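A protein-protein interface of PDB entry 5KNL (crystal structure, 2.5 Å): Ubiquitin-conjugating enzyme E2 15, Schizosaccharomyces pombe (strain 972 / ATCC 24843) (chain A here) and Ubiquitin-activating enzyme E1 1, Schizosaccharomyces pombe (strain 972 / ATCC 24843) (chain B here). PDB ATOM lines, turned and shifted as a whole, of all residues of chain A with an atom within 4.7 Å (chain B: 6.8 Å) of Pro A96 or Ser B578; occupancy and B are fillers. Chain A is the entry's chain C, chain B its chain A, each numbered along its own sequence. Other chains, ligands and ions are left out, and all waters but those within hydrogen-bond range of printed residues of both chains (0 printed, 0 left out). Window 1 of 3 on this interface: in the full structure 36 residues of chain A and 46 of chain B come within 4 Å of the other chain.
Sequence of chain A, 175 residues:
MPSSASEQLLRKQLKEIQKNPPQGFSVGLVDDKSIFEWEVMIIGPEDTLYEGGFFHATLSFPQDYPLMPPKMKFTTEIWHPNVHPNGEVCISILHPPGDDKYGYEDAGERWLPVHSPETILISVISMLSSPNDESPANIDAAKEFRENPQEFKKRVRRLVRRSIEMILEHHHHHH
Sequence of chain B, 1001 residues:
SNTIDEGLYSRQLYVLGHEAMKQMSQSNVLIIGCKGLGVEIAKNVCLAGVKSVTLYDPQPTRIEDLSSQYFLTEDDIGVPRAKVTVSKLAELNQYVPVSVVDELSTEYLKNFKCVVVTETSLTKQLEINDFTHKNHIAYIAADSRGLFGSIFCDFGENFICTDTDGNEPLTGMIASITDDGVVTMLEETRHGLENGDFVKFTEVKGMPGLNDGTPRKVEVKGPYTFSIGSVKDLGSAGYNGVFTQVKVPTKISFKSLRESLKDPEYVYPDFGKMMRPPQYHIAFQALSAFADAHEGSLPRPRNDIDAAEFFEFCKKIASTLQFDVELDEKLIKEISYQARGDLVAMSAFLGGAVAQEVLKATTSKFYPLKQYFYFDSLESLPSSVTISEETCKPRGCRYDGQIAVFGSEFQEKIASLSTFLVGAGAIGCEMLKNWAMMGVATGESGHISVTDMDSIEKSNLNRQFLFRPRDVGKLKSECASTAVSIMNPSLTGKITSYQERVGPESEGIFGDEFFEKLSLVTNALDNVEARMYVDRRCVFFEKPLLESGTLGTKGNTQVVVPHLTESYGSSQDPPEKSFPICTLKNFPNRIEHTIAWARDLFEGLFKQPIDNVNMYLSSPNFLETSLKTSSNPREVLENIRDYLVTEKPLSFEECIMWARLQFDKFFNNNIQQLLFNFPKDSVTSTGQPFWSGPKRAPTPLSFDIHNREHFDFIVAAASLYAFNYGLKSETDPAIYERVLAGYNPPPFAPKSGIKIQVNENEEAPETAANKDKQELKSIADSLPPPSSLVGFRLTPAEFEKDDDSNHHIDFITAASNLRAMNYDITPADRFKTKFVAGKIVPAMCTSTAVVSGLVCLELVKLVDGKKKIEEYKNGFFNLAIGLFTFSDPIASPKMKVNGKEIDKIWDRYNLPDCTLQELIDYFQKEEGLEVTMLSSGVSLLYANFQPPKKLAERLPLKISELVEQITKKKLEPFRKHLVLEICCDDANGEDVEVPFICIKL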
ATOM      1  N   MET A  68      18.785 -20.850  34.153  1.00  0.00           N
ATOM      2  CA  MET A  68      17.786 -19.915  33.648  1.00  0.00           C
ATOM      3  C   MET A  68      18.414 -18.542  33.447  1.00  0.00           C
ATOM      4  O   MET A  68      19.400 -18.212  34.106  1.00  0.00           O
ATOM      5  CB  MET A  68      16.609 -19.806  34.618  1.00  0.00           C
ATOM      6  CG  MET A  68      15.715 -21.029  34.686  1.00  0.00           C
ATOM      7  SD  MET A  68      14.407 -20.991  33.447  1.00  0.00           S
ATOM      8  CE  MET A  68      15.114 -22.022  32.175  1.00  0.00           C
ATOM      9  N   PRO A  69      17.842 -17.727  32.546  1.00  0.00           N
ATOM     10  CA  PRO A  69      18.397 -16.390  32.343  1.00  0.00           C
ATOM     11  C   PRO A  69      17.913 -15.412  33.401  1.00  0.00           C
ATOM     12  O   PRO A  69      16.947 -15.710  34.099  1.00  0.00           O
ATOM     13  CB  PRO A  69      17.865 -15.988  30.961  1.00  0.00           C
ATOM     14  CG  PRO A  69      16.798 -17.011  30.604  1.00  0.00           C
ATOM     15  CD  PRO A  69      16.597 -17.907  31.785  1.00  0.00           C
ATOM     16  N   LEU A  94      17.499 -13.635  26.202  1.00  0.00           N
ATOM     17  CA  LEU A  94      16.883 -13.738  27.523  1.00  0.00           C
ATOM     18  C   LEU A  94      15.683 -14.686  27.531  1.00  0.00           C
ATOM     19  O   LEU A  94      15.022 -14.843  28.558  1.00  0.00           O
ATOM     20  CB  LEU A  94      16.455 -12.355  28.016  1.00  0.00           C
ATOM     21  CG  LEU A  94      17.592 -11.389  28.361  1.00  0.00           C
ATOM     22  CD1 LEU A  94      17.032 -10.018  28.681  1.00  0.00           C
ATOM     23  CD2 LEU A  94      18.434 -11.905  29.520  1.00  0.00           C
ATOM     24  N   HIS A  95      15.403 -15.320  26.395  1.00  0.00           N
ATOM     25  CA  HIS A  95      14.317 -16.292  26.321  1.00  0.00           C
ATOM     26  C   HIS A  95      14.784 -17.605  26.936  1.00  0.00           C
ATOM     27  O   HIS A  95      15.917 -18.023  26.705  1.00  0.00           O
ATOM     28  CB  HIS A  95      13.867 -16.521  24.876  1.00  0.00           C
ATOM     29  CG  HIS A  95      13.130 -15.364  24.278  1.00  0.00           C
ATOM     30  ND1 HIS A  95      12.839 -15.284  22.932  1.00  0.00           N
ATOM     31  CD2 HIS A  95      12.615 -14.245  24.840  1.00  0.00           C
ATOM     32  CE1 HIS A  95      12.182 -14.164  22.691  1.00  0.00           C
ATOM     33  NE2 HIS A  95      12.033 -13.515  23.832  1.00  0.00           N
ATOM     34  N   PRO A  96      13.925 -18.258  27.737  1.00  0.00           N
ATOM     35  CA  PRO A  96      14.368 -19.520  28.344  1.00  0.00           C
ATOM     36  C   PRO A  96      14.696 -20.609  27.315  1.00  0.00           C
ATOM     37  O   PRO A  96      14.260 -20.509  26.168  1.00  0.00           O
ATOM     38  CB  PRO A  96      13.168 -19.936  29.201  1.00  0.00           C
ATOM     39  CG  PRO A  96      12.404 -18.683  29.441  1.00  0.00           C
ATOM     40  CD  PRO A  96      12.595 -17.848  28.221  1.00  0.00           C
ATOM     41  N   PRO A  97      15.453 -21.643  27.726  1.00  0.00           N
ATOM     42  CA  PRO A  97      15.795 -22.784  26.869  1.00  0.00           C
ATOM     43  C   PRO A  97      14.572 -23.640  26.518  1.00  0.00           C
ATOM     44  O   PRO A  97      13.720 -23.800  27.393  1.00  0.00           O
ATOM     45  CB  PRO A  97      16.794 -23.579  27.719  1.00  0.00           C
ATOM     46  CG  PRO A  97      16.577 -23.114  29.123  1.00  0.00           C
ATOM     47  CD  PRO A  97      16.190 -21.682  28.999  1.00  0.00           C
ATOM     48  N   GLY A  98      14.471 -24.183  25.302  1.00  0.00           N
ATOM     49  CA  GLY A  98      15.506 -24.109  24.281  1.00  0.00           C
ATOM     50  C   GLY A  98      14.949 -24.361  22.890  1.00  0.00           C
ATOM     51  O   GLY A  98      14.465 -23.433  22.243  1.00  0.00           O
ATOM     52  N   ARG A 110      18.933 -18.719  21.972  1.00  0.00           N
ATOM     53  CA  ARG A 110      18.321 -18.214  23.195  1.00  0.00           C
ATOM     54  C   ARG A 110      19.339 -18.200  24.336  1.00  0.00           C
ATOM     55  O   ARG A 110      20.528 -17.972  24.107  1.00  0.00           O
ATOM     56  CB  ARG A 110      17.096 -19.054  23.575  1.00  0.00           C
ATOM     57  CG  ARG A 110      16.021 -19.131  22.504  1.00  0.00           C
ATOM     58  CD  ARG A 110      14.907 -20.073  22.927  1.00  0.00           C
ATOM     59  NE  ARG A 110      13.805 -20.101  21.971  1.00  0.00           N
ATOM     60  CZ  ARG A 110      12.783 -20.950  22.032  1.00  0.00           C
ATOM     61  NH1 ARG A 110      12.720 -21.853  23.003  1.00  0.00           N
ATOM     62  NH2 ARG A 110      11.823 -20.901  21.120  1.00  0.00           N
ATOM     63  N   PRO B 575      16.753 -27.317  33.278  1.00  0.00           N
ATOM     64  CA  PRO B 575      15.661 -26.677  34.018  1.00  0.00           C
ATOM     65  C   PRO B 575      14.292 -26.907  33.387  1.00  0.00           C
ATOM     66  O   PRO B 575      14.204 -27.307  32.225  1.00  0.00           O
ATOM     67  CB  PRO B 575      16.036 -25.199  33.964  1.00  0.00           C
ATOM     68  CG  PRO B 575      16.729 -25.060  32.654  1.00  0.00           C
ATOM     69  CD  PRO B 575      17.481 -26.346  32.439  1.00  0.00           C
ATOM     70  N   GLU B 576      13.241 -26.648  34.157  1.00  0.00           N
ATOM     71  CA  GLU B 576      11.870 -26.758  33.672  1.00  0.00           C
ATOM     72  C   GLU B 576      11.576 -25.753  32.561  1.00  0.00           C
ATOM     73  O   GLU B 576      11.970 -24.590  32.636  1.00  0.00           O
ATOM     74  CB  GLU B 576      10.877 -26.566  34.819  1.00  0.00           C
ATOM     75  CG  GLU B 576      10.300 -27.868  35.349  1.00  0.00           C
ATOM     76  CD  GLU B 576       9.343 -27.654  36.506  1.00  0.00           C
ATOM     77  OE1 GLU B 576       9.735 -26.989  37.488  1.00  0.00           O
ATOM     78  OE2 GLU B 576       8.199 -28.149  36.433  1.00  0.00           O
ATOM     79  N   LYS B 577      10.881 -26.223  31.532  1.00  0.00           N
ATOM     80  CA  LYS B 577      10.542 -25.402  30.377  1.00  0.00           C
ATOM     81  C   LYS B 577       9.584 -24.277  30.758  1.00  0.00           C
ATOM     82  O   LYS B 577       8.629 -24.490  31.505  1.00  0.00           O
ATOM     83  CB  LYS B 577       9.907 -26.276  29.297  1.00  0.00           C
ATOM     84  CG  LYS B 577       9.816 -25.648  27.921  1.00  0.00           C
ATOM     85  CD  LYS B 577       9.463 -26.714  26.898  1.00  0.00           C
ATOM     86  CE  LYS B 577       9.473 -26.183  25.482  1.00  0.00           C
ATOM     87  NZ  LYS B 577       9.323 -27.298  24.509  1.00  0.00           N
ATOM     88  N   SER B 578       9.846 -23.079  30.240  1.00  0.00           N
ATOM     89  CA  SER B 578       8.998 -21.919  30.494  1.00  0.00           C
ATOM     90  C   SER B 578       8.862 -21.075  29.232  1.00  0.00           C
ATOM     91  O   SER B 578       9.537 -21.333  28.235  1.00  0.00           O
ATOM     92  CB  SER B 578       9.567 -21.078  31.637  1.00  0.00           C
ATOM     93  OG  SER B 578      10.918 -20.732  31.388  1.00  0.00           O
ATOM     94  N   PHE B 579       7.994 -20.069  29.282  1.00  0.00           N
ATOM     95  CA  PHE B 579       7.717 -19.234  28.118  1.00  0.00           C
ATOM     96  C   PHE B 579       7.754 -17.747  28.457  1.00  0.00           C
ATOM     97  O   PHE B 579       7.336 -17.347  29.542  1.00  0.00           O
ATOM     98  CB  PHE B 579       6.355 -19.599  27.529  1.00  0.00           C
ATOM     99  CG  PHE B 579       6.187 -21.067  27.272  1.00  0.00           C
ATOM    100  CD1 PHE B 579       6.718 -21.648  26.132  1.00  0.00           C
ATOM    101  CD2 PHE B 579       5.516 -21.867  28.177  1.00  0.00           C
ATOM    102  CE1 PHE B 579       6.570 -23.002  25.893  1.00  0.00           C
ATOM    103  CE2 PHE B 579       5.366 -23.221  27.946  1.00  0.00           C
ATOM    104  CZ  PHE B 579       5.895 -23.790  26.803  1.00  0.00           C
ATOM    105  N   PRO B 580       8.251 -16.918  27.523  1.00  0.00           N
ATOM    106  CA  PRO B 580       8.284 -15.467  27.743  1.00  0.00           C
ATOM    107  C   PRO B 580       6.902 -14.831  27.605  1.00  0.00           C
ATOM    108  O   PRO B 580       6.049 -15.379  26.912  1.00  0.00           O
ATOM    109  CB  PRO B 580       9.230 -14.973  26.648  1.00  0.00           C
ATOM    110  CG  PRO B 580       9.075 -15.963  25.553  1.00  0.00           C
ATOM    111  CD  PRO B 580       8.836 -17.286  26.221  1.00  0.00           C
ATOM    112  N   GLU B 592       0.175 -25.174  24.762  1.00  0.00           N
ATOM    113  CA  GLU B 592       0.867 -24.890  26.011  1.00  0.00           C
ATOM    114  C   GLU B 592       0.974 -23.384  26.244  1.00  0.00           C
ATOM    115  O   GLU B 592       1.008 -22.929  27.387  1.00  0.00           O
ATOM    116  CB  GLU B 592       2.253 -25.534  26.005  1.00  0.00           C
ATOM    117  CG  GLU B 592       2.824 -25.770  27.397  1.00  0.00           C
ATOM    118  CD  GLU B 592       3.725 -26.992  27.474  1.00  0.00           C
ATOM    119  OE1 GLU B 592       3.436 -28.001  26.797  1.00  0.00           O
ATOM    120  OE2 GLU B 592       4.722 -26.944  28.225  1.00  0.00           O
ATOM    121  N   HIS B 593       1.020 -22.615  25.159  1.00  0.00           N
ATOM    122  CA  HIS B 593       1.050 -21.160  25.258  1.00  0.00           C
ATOM    123  C   HIS B 593      -0.292 -20.620  25.737  1.00  0.00           C
ATOM    124  O   HIS B 593      -0.346 -19.745  26.602  1.00  0.00           O
ATOM    125  CB  HIS B 593       1.409 -20.526  23.910  1.00  0.00           C
ATOM    126  CG  HIS B 593       2.833 -20.734  23.501  1.00  0.00           C
ATOM    127  ND1 HIS B 593       3.266 -20.565  22.205  1.00  0.00           N
ATOM    128  CD2 HIS B 593       3.923 -21.094  24.218  1.00  0.00           C
ATOM    129  CE1 HIS B 593       4.560 -20.815  22.140  1.00  0.00           C
ATOM    130  NE2 HIS B 593       4.985 -21.137  23.348  1.00  0.00           N
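Ser B578 touches one residue of chain A.
Printed residues of chain A within 4 Å of Pro B575: Met A68.
Of the printed residues of chain B, Met A68 touches Pro B575 (3.5 Å).
Pro A97 touches none of the printed residues of chain B.
The nearest residue of chain A that does not touch Ser B578 is Met A68 (4.1 Å).
Pro B575 touches Met A68.
His A95 touches Pro B580 (CD2 to CB, 3.9 Å).
Pro A96 touches Ser B578.
Hydrophobic or aromatic side chains of chain A within 4 Å of the printed part of chain B: Met A68, His A95 and Pro A96.
Of the 8 printed residues of chain B, 3 touch a printed residue of chain A.
Printed residues of chain B that touch a printed residue of chain A: Pro B575, Ser B578 and Pro B580.
Along chain B the printed residues that touch a printed residue of chain A span positions 575 to 580.
Among the printed residues, 3 pairs touch across the chains.
Among the printed residues, no Asp or Glu carboxylate lies within 4 Å of a Lys or Arg side-chain nitrogen of the other chain.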
